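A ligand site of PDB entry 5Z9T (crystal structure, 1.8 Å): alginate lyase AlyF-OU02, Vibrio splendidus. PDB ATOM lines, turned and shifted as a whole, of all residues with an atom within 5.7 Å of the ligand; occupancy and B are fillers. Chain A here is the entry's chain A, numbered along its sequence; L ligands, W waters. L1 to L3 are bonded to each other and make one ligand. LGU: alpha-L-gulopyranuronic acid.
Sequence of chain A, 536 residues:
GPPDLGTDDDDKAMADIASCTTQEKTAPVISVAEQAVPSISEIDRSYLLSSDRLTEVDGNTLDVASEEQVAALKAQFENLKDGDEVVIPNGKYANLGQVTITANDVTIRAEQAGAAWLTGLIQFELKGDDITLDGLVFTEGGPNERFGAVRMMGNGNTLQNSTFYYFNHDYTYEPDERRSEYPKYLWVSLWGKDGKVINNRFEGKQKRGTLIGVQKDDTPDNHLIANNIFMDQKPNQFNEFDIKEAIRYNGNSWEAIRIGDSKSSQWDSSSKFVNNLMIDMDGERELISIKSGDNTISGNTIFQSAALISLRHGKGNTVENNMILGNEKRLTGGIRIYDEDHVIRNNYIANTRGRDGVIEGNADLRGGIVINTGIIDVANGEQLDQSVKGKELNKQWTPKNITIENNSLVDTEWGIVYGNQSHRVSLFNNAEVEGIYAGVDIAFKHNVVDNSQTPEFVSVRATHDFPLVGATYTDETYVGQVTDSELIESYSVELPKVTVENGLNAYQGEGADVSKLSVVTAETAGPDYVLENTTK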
ATOM      1  N   ARG A 146      -7.966  15.113   2.245  1.00  0.00           N
ATOM      2  CA  ARG A 146      -6.490  14.997   2.181  1.00  0.00           C
ATOM      3  C   ARG A 146      -5.902  13.612   2.051  1.00  0.00           C
ATOM      4  O   ARG A 146      -4.699  13.487   1.691  1.00  0.00           O
ATOM      5  CB  ARG A 146      -5.769  15.755   3.321  1.00  0.00           C
ATOM      6  CG  ARG A 146      -5.641  15.036   4.662  1.00  0.00           C
ATOM      7  CD  ARG A 146      -5.003  15.955   5.683  1.00  0.00           C
ATOM      8  NE  ARG A 146      -4.488  15.189   6.826  1.00  0.00           N
ATOM      9  CZ  ARG A 146      -3.355  14.485   6.844  1.00  0.00           C
ATOM     10  NH1 ARG A 146      -2.540  14.429   5.784  1.00  0.00           N
ATOM     11  NH2 ARG A 146      -3.005  13.848   7.988  1.00  0.00           N
ATOM     12  N   PHE A 147      -6.694  12.579   2.350  1.00  0.00           N
ATOM     13  CA  PHE A 147      -6.224  11.194   2.135  1.00  0.00           C
ATOM     14  C   PHE A 147      -6.363  10.665   0.710  1.00  0.00           C
ATOM     15  O   PHE A 147      -6.118   9.461   0.477  1.00  0.00           O
ATOM     16  CB  PHE A 147      -6.690  10.212   3.252  1.00  0.00           C
ATOM     17  CG  PHE A 147      -5.904  10.390   4.534  1.00  0.00           C
ATOM     18  CD1 PHE A 147      -4.692   9.706   4.715  1.00  0.00           C
ATOM     19  CD2 PHE A 147      -6.330  11.294   5.516  1.00  0.00           C
ATOM     20  CE1 PHE A 147      -3.944   9.904   5.888  1.00  0.00           C
ATOM     21  CE2 PHE A 147      -5.570  11.510   6.686  1.00  0.00           C
ATOM     22  CZ  PHE A 147      -4.376  10.795   6.867  1.00  0.00           C
ATOM     23  N   LYS A 184      -0.687  18.340   4.186  1.00  0.00           N
ATOM     24  CA  LYS A 184      -0.260  17.139   3.469  1.00  0.00           C
ATOM     25  C   LYS A 184      -1.471  16.538   2.757  1.00  0.00           C
ATOM     26  O   LYS A 184      -2.422  16.066   3.398  1.00  0.00           O
ATOM     27  CB  LYS A 184       0.308  16.112   4.485  1.00  0.00           C
ATOM     28  CG  LYS A 184       1.589  16.581   5.223  1.00  0.00           C
ATOM     29  CD  LYS A 184       1.914  15.535   6.319  1.00  0.00           C
ATOM     30  CE  LYS A 184       1.054  15.818   7.568  1.00  0.00           C
ATOM     31  NZ  LYS A 184       1.114  14.613   8.439  1.00  0.00           N
ATOM     32  N   LEU A 186      -2.444  13.510   0.142  1.00  0.00           N
ATOM     33  CA  LEU A 186      -2.005  12.275  -0.526  1.00  0.00           C
ATOM     34  C   LEU A 186      -2.707  12.135  -1.845  1.00  0.00           C
ATOM     35  O   LEU A 186      -3.714  12.800  -2.062  1.00  0.00           O
ATOM     36  CB  LEU A 186      -2.364  11.056   0.378  1.00  0.00           C
ATOM     37  CG  LEU A 186      -1.492  10.900   1.632  1.00  0.00           C
ATOM     38  CD1 LEU A 186      -1.698  12.012   2.661  1.00  0.00           C
ATOM     39  CD2 LEU A 186      -1.781   9.527   2.218  1.00  0.00           C
ATOM     40  N   ARG A 208       2.874  19.303  -0.984  1.00  0.00           N
ATOM     41  CA  ARG A 208       3.290  18.457   0.167  1.00  0.00           C
ATOM     42  C   ARG A 208       2.363  17.230   0.374  1.00  0.00           C
ATOM     43  O   ARG A 208       1.129  17.297   0.159  1.00  0.00           O
ATOM     44  CB  ARG A 208       3.317  19.324   1.446  1.00  0.00           C
ATOM     45  CG  ARG A 208       4.062  18.720   2.630  1.00  0.00           C
ATOM     46  CD  ARG A 208       4.267  19.734   3.745  1.00  0.00           C
ATOM     47  NE  ARG A 208       4.954  19.078   4.862  1.00  0.00           N
ATOM     48  CZ  ARG A 208       4.396  18.847   6.052  1.00  0.00           C
ATOM     49  NH1 ARG A 208       3.157  19.312   6.332  1.00  0.00           N
ATOM     50  NH2 ARG A 208       5.101  18.189   6.995  1.00  0.00           N
ATOM     51  N   THR A 210       2.802  12.616   1.208  1.00  0.00           N
ATOM     52  CA  THR A 210       3.187  11.347   0.534  1.00  0.00           C
ATOM     53  C   THR A 210       2.214  11.016  -0.639  1.00  0.00           C
ATOM     54  O   THR A 210       1.018  11.301  -0.569  1.00  0.00           O
ATOM     55  CB  THR A 210       3.286  10.191   1.562  1.00  0.00           C
ATOM     56  OG1 THR A 210       3.849   9.051   0.872  1.00  0.00           O
ATOM     57  CG2 THR A 210       1.903   9.816   2.072  1.00  0.00           C
ATOM     58  N   GLN A 215      -2.156   3.261   5.804  1.00  0.00           N
ATOM     59  CA  GLN A 215      -2.619   3.538   7.160  1.00  0.00           C
ATOM     60  C   GLN A 215      -3.093   2.141   7.636  1.00  0.00           C
ATOM     61  O   GLN A 215      -4.107   1.640   7.138  1.00  0.00           O
ATOM     62  CB  GLN A 215      -3.855   4.440   7.046  1.00  0.00           C
ATOM     63  CG  GLN A 215      -3.689   5.669   6.157  1.00  0.00           C
ATOM     64  CD  GLN A 215      -2.401   6.407   6.475  1.00  0.00           C
ATOM     65  OE1 GLN A 215      -1.535   6.581   5.613  1.00  0.00           O
ATOM     66  NE2 GLN A 215      -2.249   6.817   7.749  1.00  0.00           N
ATOM     67  N   ASN A 252       9.580  18.105   4.766  1.00  0.00           N
ATOM     68  CA  ASN A 252       9.328  16.679   5.101  1.00  0.00           C
ATOM     69  C   ASN A 252       7.937  16.284   4.620  1.00  0.00           C
ATOM     70  O   ASN A 252       7.098  17.175   4.418  1.00  0.00           O
ATOM     71  CB  ASN A 252       9.366  16.408   6.623  1.00  0.00           C
ATOM     72  CG  ASN A 252       9.462  14.924   6.934  1.00  0.00           C
ATOM     73  OD1 ASN A 252      10.258  14.214   6.289  1.00  0.00           O
ATOM     74  ND2 ASN A 252       8.718  14.437   7.922  1.00  0.00           N
ATOM     75  N   SER A 253       7.708  14.973   4.458  1.00  0.00           N
ATOM     76  CA  SER A 253       6.445  14.418   3.954  1.00  0.00           C
ATOM     77  C   SER A 253       6.210  14.674   2.453  1.00  0.00           C
ATOM     78  O   SER A 253       5.135  15.089   2.054  1.00  0.00           O
ATOM     79  CB  SER A 253       5.218  14.788   4.848  1.00  0.00           C
ATOM     80  OG  SER A 253       5.588  14.464   6.220  1.00  0.00           O
ATOM     81  N   GLU A 255       7.143  11.896   0.403  1.00  0.00           N
ATOM     82  CA  GLU A 255       7.616  10.553  -0.079  1.00  0.00           C
ATOM     83  C   GLU A 255       6.799  10.099  -1.293  1.00  0.00           C
ATOM     84  O   GLU A 255       5.667  10.548  -1.487  1.00  0.00           O
ATOM     85  CB  GLU A 255       7.397   9.504   1.008  1.00  0.00           C
ATOM     86  CG  GLU A 255       8.163   9.790   2.325  1.00  0.00           C
ATOM     87  CD  GLU A 255       7.369  10.650   3.358  1.00  0.00           C
ATOM     88  OE1 GLU A 255       6.285  11.203   3.058  1.00  0.00           O
ATOM     89  OE2 GLU A 255       7.859  10.740   4.527  1.00  0.00           O
ATOM     90  N   ARG A 258       4.634   5.824   1.725  1.00  0.00           N
ATOM     91  CA  ARG A 258       4.923   5.649   3.173  1.00  0.00           C
ATOM     92  C   ARG A 258       4.136   4.418   3.577  1.00  0.00           C
ATOM     93  O   ARG A 258       2.898   4.409   3.419  1.00  0.00           O
ATOM     94  CB  ARG A 258       4.422   6.842   3.991  1.00  0.00           C
ATOM     95  CG  ARG A 258       4.564   6.622   5.513  1.00  0.00           C
ATOM     96  CD  ARG A 258       3.989   7.778   6.342  1.00  0.00           C
ATOM     97  NE  ARG A 258       2.752   8.363   5.826  1.00  0.00           N
ATOM     98  CZ  ARG A 258       1.570   7.750   5.752  1.00  0.00           C
ATOM     99  NH1 ARG A 258       1.420   6.508   6.189  1.00  0.00           N
ATOM    100  NH2 ARG A 258       0.503   8.410   5.223  1.00  0.00           N
ATOM    101  N   GLY A 260       2.922   2.503   6.592  1.00  0.00           N
ATOM    102  CA  GLY A 260       2.767   2.468   8.064  1.00  0.00           C
ATOM    103  C   GLY A 260       3.028   3.862   8.585  1.00  0.00           C
ATOM    104  O   GLY A 260       3.196   4.823   7.828  1.00  0.00           O
ATOM    105  N   ASP A 261       3.097   3.984   9.916  1.00  0.00           N
ATOM    106  CA  ASP A 261       3.394   5.264  10.527  1.00  0.00           C
ATOM    107  C   ASP A 261       3.966   4.985  11.919  1.00  0.00           C
ATOM    108  O   ASP A 261       4.058   3.814  12.300  1.00  0.00           O
ATOM    109  CB  ASP A 261       2.190   6.250  10.548  1.00  0.00           C
ATOM    110  CG  ASP A 261       0.969   5.727  11.332  1.00  0.00           C
ATOM    111  OD1 ASP A 261       1.016   4.730  12.102  1.00  0.00           O
ATOM    112  OD2 ASP A 261      -0.069   6.400  11.188  1.00  0.00           O
ATOM    113  N   SER A 262       4.412   6.013  12.609  1.00  0.00           N
ATOM    114  CA  SER A 262       5.132   5.755  13.880  1.00  0.00           C
ATOM    115  C   SER A 262       4.281   4.944  14.856  1.00  0.00           C
ATOM    116  O   SER A 262       4.772   3.998  15.474  1.00  0.00           O
ATOM    117  CB  SER A 262       5.597   7.070  14.483  1.00  0.00           C
ATOM    118  OG  SER A 262       4.510   7.939  14.786  1.00  0.00           O
ATOM    119  N   LYS A 263       2.972   5.280  14.964  1.00  0.00           N
ATOM    120  CA  LYS A 263       2.130   4.528  15.945  1.00  0.00           C
ATOM    121  C   LYS A 263       1.968   3.045  15.590  1.00  0.00           C
ATOM    122  O   LYS A 263       1.886   2.196  16.478  1.00  0.00           O
ATOM    123  CB  LYS A 263       0.705   5.154  16.055  1.00  0.00           C
ATOM    124  N   GLU A 284      11.916  14.357  -1.203  1.00  0.00           N
ATOM    125  CA  GLU A 284      12.575  14.626   0.076  1.00  0.00           C
ATOM    126  C   GLU A 284      13.665  13.575   0.328  1.00  0.00           C
ATOM    127  O   GLU A 284      13.900  12.698  -0.502  1.00  0.00           O
ATOM    128  CB  GLU A 284      11.523  14.589   1.208  1.00  0.00           C
ATOM    129  CG  GLU A 284      10.815  13.234   1.284  1.00  0.00           C
ATOM    130  CD  GLU A 284      10.489  12.868   2.706  1.00  0.00           C
ATOM    131  OE1 GLU A 284      11.393  12.347   3.402  1.00  0.00           O
ATOM    132  OE2 GLU A 284       9.349  13.127   3.161  1.00  0.00           O
ATOM    133  N   ARG A 285      14.265  13.560   1.523  1.00  0.00           N
ATOM    134  CA  ARG A 285      15.302  12.597   1.767  1.00  0.00           C
ATOM    135  C   ARG A 285      14.812  11.132   1.637  1.00  0.00           C
ATOM    136  O   ARG A 285      15.590  10.255   1.226  1.00  0.00           O
ATOM    137  CB  ARG A 285      15.978  12.856   3.127  1.00  0.00           C
ATOM    138  CG  ARG A 285      15.096  12.586   4.309  1.00  0.00           C
ATOM    139  CD  ARG A 285      15.602  13.135   5.689  1.00  0.00           C
ATOM    140  NE  ARG A 285      14.605  12.710   6.675  1.00  0.00           N
ATOM    141  CZ  ARG A 285      13.362  13.204   6.722  1.00  0.00           C
ATOM    142  NH1 ARG A 285      13.014  14.252   5.962  1.00  0.00           N
ATOM    143  NH2 ARG A 285      12.481  12.687   7.550  1.00  0.00           N
ATOM    144  N   GLU A 286      13.532  10.889   1.963  1.00  0.00           N
ATOM    145  CA  GLU A 286      12.947   9.536   1.849  1.00  0.00           C
ATOM    146  C   GLU A 286      12.130   9.419   0.589  1.00  0.00           C
ATOM    147  O   GLU A 286      11.116  10.094   0.453  1.00  0.00           O
ATOM    148  CB  GLU A 286      12.014   9.232   3.049  1.00  0.00           C
ATOM    149  CG  GLU A 286      12.761   9.394   4.384  1.00  0.00           C
ATOM    150  CD  GLU A 286      11.845   9.022   5.558  1.00  0.00           C
ATOM    151  OE1 GLU A 286      10.995   9.874   5.920  1.00  0.00           O
ATOM    152  OE2 GLU A 286      11.947   7.881   6.078  1.00  0.00           O
ATOM    153  N   SER A 289       9.311   5.525   2.438  1.00  0.00           N
ATOM    154  CA  SER A 289       9.507   5.531   3.913  1.00  0.00           C
ATOM    155  C   SER A 289       8.797   4.330   4.510  1.00  0.00           C
ATOM    156  O   SER A 289       7.579   4.305   4.560  1.00  0.00           O
ATOM    157  CB  SER A 289       8.938   6.834   4.510  1.00  0.00           C
ATOM    158  OG  SER A 289       9.159   6.832   5.927  1.00  0.00           O
ATOM    159  N   LYS A 291       7.628   2.304   7.551  1.00  0.00           N
ATOM    160  CA  LYS A 291       7.330   2.591   8.980  1.00  0.00           C
ATOM    161  C   LYS A 291       6.446   1.460   9.534  1.00  0.00           C
ATOM    162  O   LYS A 291       5.387   1.720  10.115  1.00  0.00           O
ATOM    163  CB  LYS A 291       6.604   3.933   9.045  1.00  0.00           C
ATOM    164  CG  LYS A 291       7.461   5.090   8.586  1.00  0.00           C
ATOM    165  CD  LYS A 291       6.600   6.354   8.811  1.00  0.00           C
ATOM    166  CE  LYS A 291       7.398   7.482   9.387  1.00  0.00           C
ATOM    167  NZ  LYS A 291       6.477   8.683   9.304  1.00  0.00           N
ATOM    168  N   ARG A 312      12.655   3.474   8.047  1.00  0.00           N
ATOM    169  CA  ARG A 312      12.580   4.611   8.980  1.00  0.00           C
ATOM    170  C   ARG A 312      12.139   4.124  10.381  1.00  0.00           C
ATOM    171  O   ARG A 312      12.787   4.492  11.391  1.00  0.00           O
ATOM    172  CB  ARG A 312      11.604   5.640   8.445  1.00  0.00           C
ATOM    173  CG  ARG A 312      11.431   6.813   9.413  1.00  0.00           C
ATOM    174  CD  ARG A 312      12.715   7.645   9.576  1.00  0.00           C
ATOM    175  NE  ARG A 312      12.505   8.698  10.586  1.00  0.00           N
ATOM    176  CZ  ARG A 312      12.602   8.487  11.922  1.00  0.00           C
ATOM    177  NH1 ARG A 312      12.944   7.289  12.381  1.00  0.00           N
ATOM    178  NH2 ARG A 312      12.372   9.503  12.774  1.00  0.00           N
ATOM    179  N   HIS A 313      11.086   3.297  10.410  1.00  0.00           N
ATOM    180  CA  HIS A 313      10.664   2.586  11.673  1.00  0.00           C
ATOM    181  C   HIS A 313      10.229   1.180  11.332  1.00  0.00           C
ATOM    182  O   HIS A 313       9.791   0.880  10.173  1.00  0.00           O
ATOM    183  CB  HIS A 313       9.428   3.240  12.336  1.00  0.00           C
ATOM    184  CG  HIS A 313       9.457   4.739  12.533  1.00  0.00           C
ATOM    185  ND1 HIS A 313      10.381   5.387  13.321  1.00  0.00           N
ATOM    186  CD2 HIS A 313       8.506   5.671  12.228  1.00  0.00           C
ATOM    187  CE1 HIS A 313      10.067   6.672  13.391  1.00  0.00           C
ATOM    188  NE2 HIS A 313       8.939   6.868  12.747  1.00  0.00           N
ATOM    189  N   ARG A 336      18.907   4.105   3.338  1.00  0.00           N
ATOM    190  CA  ARG A 336      19.275   4.560   4.703  1.00  0.00           C
ATOM    191  C   ARG A 336      18.457   3.757   5.706  1.00  0.00           C
ATOM    192  O   ARG A 336      17.298   3.368   5.417  1.00  0.00           O
ATOM    193  CB  ARG A 336      19.051   6.062   4.829  1.00  0.00           C
ATOM    194  CG  ARG A 336      17.583   6.482   4.720  1.00  0.00           C
ATOM    195  CD  ARG A 336      17.419   8.027   4.696  1.00  0.00           C
ATOM    196  NE  ARG A 336      17.816   8.746   5.903  1.00  0.00           N
ATOM    197  CZ  ARG A 336      17.004   9.186   6.883  1.00  0.00           C
ATOM    198  NH1 ARG A 336      15.695   8.908   6.928  1.00  0.00           N
ATOM    199  NH2 ARG A 336      17.529   9.943   7.836  1.00  0.00           N
ATOM    200  N   LEU A 393       7.972   6.455  19.696  1.00  0.00           N
ATOM    201  CA  LEU A 393       8.049   5.581  18.534  1.00  0.00           C
ATOM    202  C   LEU A 393       8.370   6.398  17.256  1.00  0.00           C
ATOM    203  O   LEU A 393       8.791   5.802  16.224  1.00  0.00           O
ATOM    204  CB  LEU A 393       6.701   4.836  18.353  1.00  0.00           C
ATOM    205  CG  LEU A 393       6.341   3.755  19.406  1.00  0.00           C
ATOM    206  CD1 LEU A 393       5.020   3.065  19.056  1.00  0.00           C
ATOM    207  CD2 LEU A 393       7.489   2.756  19.612  1.00  0.00           C
ATOM    208  N   ASN A 394       8.130   7.720  17.279  1.00  0.00           N
ATOM    209  CA  ASN A 394       8.434   8.511  16.083  1.00  0.00           C
ATOM    210  C   ASN A 394       9.893   9.020  16.076  1.00  0.00           C
ATOM    211  O   ASN A 394      10.259   9.798  15.230  1.00  0.00           O
ATOM    212  CB  ASN A 394       7.449   9.677  15.872  1.00  0.00           C
ATOM    213  CG  ASN A 394       7.559  10.722  16.962  1.00  0.00           C
ATOM    214  OD1 ASN A 394       7.855  10.398  18.107  1.00  0.00           O
ATOM    215  ND2 ASN A 394       7.389  11.971  16.594  1.00  0.00           N
ATOM    216  N   LYS A 395      10.712   8.558  17.036  1.00  0.00           N
ATOM    217  CA  LYS A 395      12.088   9.035  17.112  1.00  0.00           C
ATOM    218  C   LYS A 395      13.023   8.118  16.290  1.00  0.00           C
ATOM    219  O   LYS A 395      12.605   7.605  15.271  1.00  0.00           O
ATOM    220  CB  LYS A 395      12.492   9.207  18.591  1.00  0.00           C
ATOM    221  CG  LYS A 395      11.547  10.199  19.285  1.00  0.00           C
ATOM    222  CD  LYS A 395      11.373  11.537  18.567  1.00  0.00           C
ATOM    223  CE  LYS A 395      10.361  12.481  19.266  1.00  0.00           C
ATOM    224  NZ  LYS A 395      10.907  13.000  20.576  1.00  0.00           N
ATOM    225  N   LEU A 427      10.470  17.210  14.756  1.00  0.00           N
ATOM    226  CA  LEU A 427      10.519  18.045  13.533  1.00  0.00           C
ATOM    227  C   LEU A 427      10.231  19.494  13.904  1.00  0.00           C
ATOM    228  O   LEU A 427      10.579  20.415  13.155  1.00  0.00           O
ATOM    229  CB  LEU A 427       9.452  17.582  12.517  1.00  0.00           C
ATOM    230  CG  LEU A 427       9.787  16.232  11.845  1.00  0.00           C
ATOM    231  CD1 LEU A 427       8.529  15.708  11.082  1.00  0.00           C
ATOM    232  CD2 LEU A 427      10.962  16.444  10.882  1.00  0.00           C
HETATM  233  C1  LGU L   1      -0.990  11.564  10.097  1.00  0.00           C
HETATM  234  C2  LGU L   1      -0.086  10.487  10.688  1.00  0.00           C
HETATM  235  O2  LGU L   1      -0.656   9.895  11.845  1.00  0.00           O
HETATM  236  C3  LGU L   1       0.579   9.497   9.703  1.00  0.00           C
HETATM  237  O3  LGU L   1      -0.287   8.395   9.426  1.00  0.00           O
HETATM  238  C4  LGU L   1       0.911  10.263   8.411  1.00  0.00           C
HETATM  239  O4  LGU L   1       1.817  11.329   8.721  1.00  0.00           O
HETATM  240  C5  LGU L   1      -0.335  10.911   7.812  1.00  0.00           C
HETATM  241  O5  LGU L   1      -1.076  11.760   8.698  1.00  0.00           O
HETATM  242  C6  LGU L   1       0.014  11.754   6.611  1.00  0.00           C
HETATM  243  O6B LGU L   1      -0.283  12.977   6.588  1.00  0.00           O
HETATM  244  O6A LGU L   1       0.582  11.178   5.684  1.00  0.00           O
HETATM  245  O1  LGU L   1      -2.233  11.974  10.702  1.00  0.00           O
HETATM  246  C1  LGU L   2       3.183  10.923   8.496  1.00  0.00           C
HETATM  247  C2  LGU L   2       4.081  12.141   8.399  1.00  0.00           C
HETATM  248  O2  LGU L   2       3.539  13.054   7.425  1.00  0.00           O
HETATM  249  C3  LGU L   2       4.335  12.845   9.757  1.00  0.00           C
HETATM  250  O3  LGU L   2       3.186  13.585  10.124  1.00  0.00           O
HETATM  251  C4  LGU L   2       4.687  11.853  10.872  1.00  0.00           C
HETATM  252  O4  LGU L   2       6.025  11.329  10.625  1.00  0.00           O
HETATM  253  C5  LGU L   2       3.714  10.675  10.825  1.00  0.00           C
HETATM  254  O5  LGU L   2       3.664  10.056   9.518  1.00  0.00           O
HETATM  255  C6  LGU L   2       4.106   9.625  11.817  1.00  0.00           C
HETATM  256  O6B LGU L   2       4.325   9.943  13.014  1.00  0.00           O
HETATM  257  O6A LGU L   2       4.387   8.501  11.397  1.00  0.00           O
HETATM  258  C1  LGU L   3       7.149  12.202  10.913  1.00  0.00           C
HETATM  259  C2  LGU L   3       7.784  11.732  12.237  1.00  0.00           C
HETATM  260  O2  LGU L   3       6.762  11.739  13.247  1.00  0.00           O
HETATM  261  C3  LGU L   3       8.475  10.340  12.150  1.00  0.00           C
HETATM  262  O3  LGU L   3       7.524   9.245  12.189  1.00  0.00           O
HETATM  263  C4  LGU L   3       9.375  10.276  10.886  1.00  0.00           C
HETATM  264  C5  LGU L   3       8.664  10.842   9.675  1.00  0.00           C
HETATM  265  O5  LGU L   3       8.149  12.170   9.888  1.00  0.00           O
HETATM  266  C6  LGU L   3       9.520  10.814   8.428  1.00  0.00           C
HETATM  267  O6B LGU L   3       9.385  11.716   7.564  1.00  0.00           O
HETATM  268  O6A LGU L   3      10.283   9.813   8.284  1.00  0.00           O
HETATM  269  O   HOH W   1      -4.620  12.540  10.260  1.00  0.00           O
HETATM  270  O   HOH W   2       4.335  11.047   4.953  1.00  0.00           O
HETATM  271  O   HOH W   3      -1.442   6.986  13.507  1.00  0.00           O
HETATM  272  O   HOH W   4       4.257  15.595  11.803  1.00  0.00           O
HETATM  273  O   HOH W   5      -0.412  14.760  10.560  1.00  0.00           O
HETATM  274  O   HOH W   6       3.596  12.218  14.388  1.00  0.00           O
HETATM  275  O   HOH W   7       6.073  14.493  13.771  1.00  0.00           O
HETATM  276  O   HOH W   8       2.059  12.724   3.950  1.00  0.00           O
HETATM  277  O   HOH W   9       6.747  12.155   6.423  1.00  0.00           O
HETATM  278  O   HOH W  10       7.369   8.875   6.551  1.00  0.00           O
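OE1 of Glu 284 lies within hydrogen-bond range of N of Glu 286. The guanidinium group (NH1) of Arg 146 lies within hydrogen-bond range of the backbone carbonyl oxygen (O) of Lys 184 (2.9 Å). O of Arg 146 is in hydrogen-bond range of N of Leu 186. The backbone NH of Arg 258 lies within hydrogen-bond range of the side-chain hydroxyl of Thr 210 (3.4 Å). The guanidinium group (NH1) of Arg 258 lies within hydrogen-bond range of the backbone carbonyl oxygen (O) of Gly 260, 2.9 Å away. A ring nitrogen (ND1) of His 313 sits close to the guanidinium group (NH1) of Arg 312, 3.3 Å away. ND1 of His 313 sits close to O of Leu 393, at 3.3 Å. OD1 of Asn 252 lies close to OE2 of Glu 284 (3.4 Å).
OE1 of Glu 286 lies close to O6A of LGU L3 (2.5 Å). The side-chain carboxylate (OD2) of Asp 261 is in hydrogen-bond range of an oxygen (O3) of LGU L1. The backbone NH (N) of Ser 262 sits at hydrogen-bond distance from an oxygen (O6A) of LGU L2, at 2.8 Å. The side-chain hydroxyl (OG) of Ser 262 is in hydrogen-bond range of an oxygen (O6B) of LGU L2 (2.7 Å). The side-chain hydroxyl (OG) of Ser 253 is in hydrogen-bond range of an oxygen (O2) of LGU L2 (2.8 Å). O6B of LGU L1 is in salt-bridge range of NH1 of Arg 146, at 2.8 Å. The guanidinium group (NH2) of Arg 258 lies within salt-bridge range of an oxygen (O6A) of LGU L1, 2.8 Å away. NE2 of His 313 sits at hydrogen-bond distance from O3 of LGU L3 (2.8 Å). An oxygen (O6B) of LGU L3 sits at hydrogen-bond distance from the side-chain amide nitrogen (ND2) of Asn 252. NZ of Lys 184 is in salt-bridge range of O6B of LGU L1, 2.8 Å away. NZ of Lys 291 is in salt-bridge range of O6A of LGU L2 (3.0 Å). An oxygen (O3) of LGU L1 sits at hydrogen-bond distance from the side-chain amide nitrogen (NE2) of Gln 215 (3.0 Å). NH2 of Arg 285 lies within salt-bridge range of O6B of LGU L3, 3.2 Å away. The guanidinium group of Arg 312 is in salt-bridge range of an oxygen (O6A) of LGU L3, 3.4 Å away. The side-chain amide nitrogen of Asn 394 lies close to an oxygen (O2) of LGU L3, 3.4 Å away.
Water W1 lies within hydrogen-bond range of an oxygen (O1) of LGU L1 and the guanidinium group (NH2) of Arg 146. Water W8 lies within hydrogen-bond range of an oxygen (O6A) of LGU L1 (2.8 Å) and the backbone NH of Thr 210 (2.8 Å). Water W9 lies within hydrogen-bond range of the side-chain hydroxyl (OG) of Ser 253 (2.6 Å), the side-chain carboxylate (OE2) of Glu 255 (2.6 Å), an oxygen (O6B) of LGU L3 (2.9 Å) and the side-chain amide nitrogen (ND2) of Asn 252 (3.4 Å). Water W5 lies within hydrogen-bond range of NZ of Lys 184 and O1 of LGU L1. Water W2 lies within hydrogen-bond range of the side-chain carboxylate of Glu 255, the guanidinium group of Arg 258 and an oxygen (O2) of LGU L2. Water W10 lies within hydrogen-bond range of OG of Ser 289, OE2 of Glu 255 and NZ of Lys 291.
Phe 147 touches the ligand. Leu 186 touches the ligand. Glu 255 touches the ligand. OG of Ser 289 touches O6A of LGU L3 (3.96 Å). CD1 of Leu 427 touches O5 of LGU L3, at 3.8 Å. Hydrophobic or aromatic side chains that line the ligand: Phe 147, Leu 186, His 313 and Leu 427. 19 residues have an atom within 4 Å of the ligand: Arg 146, Phe 147, Lys 184, Leu 186, Gln 215, Asn 252, Ser 253, Glu 255, Arg 258, Asp 261, Ser 262, Arg 285, Glu 286, Ser 289, Lys 291, Arg 312, His 313, Asn 394 and Leu 427.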
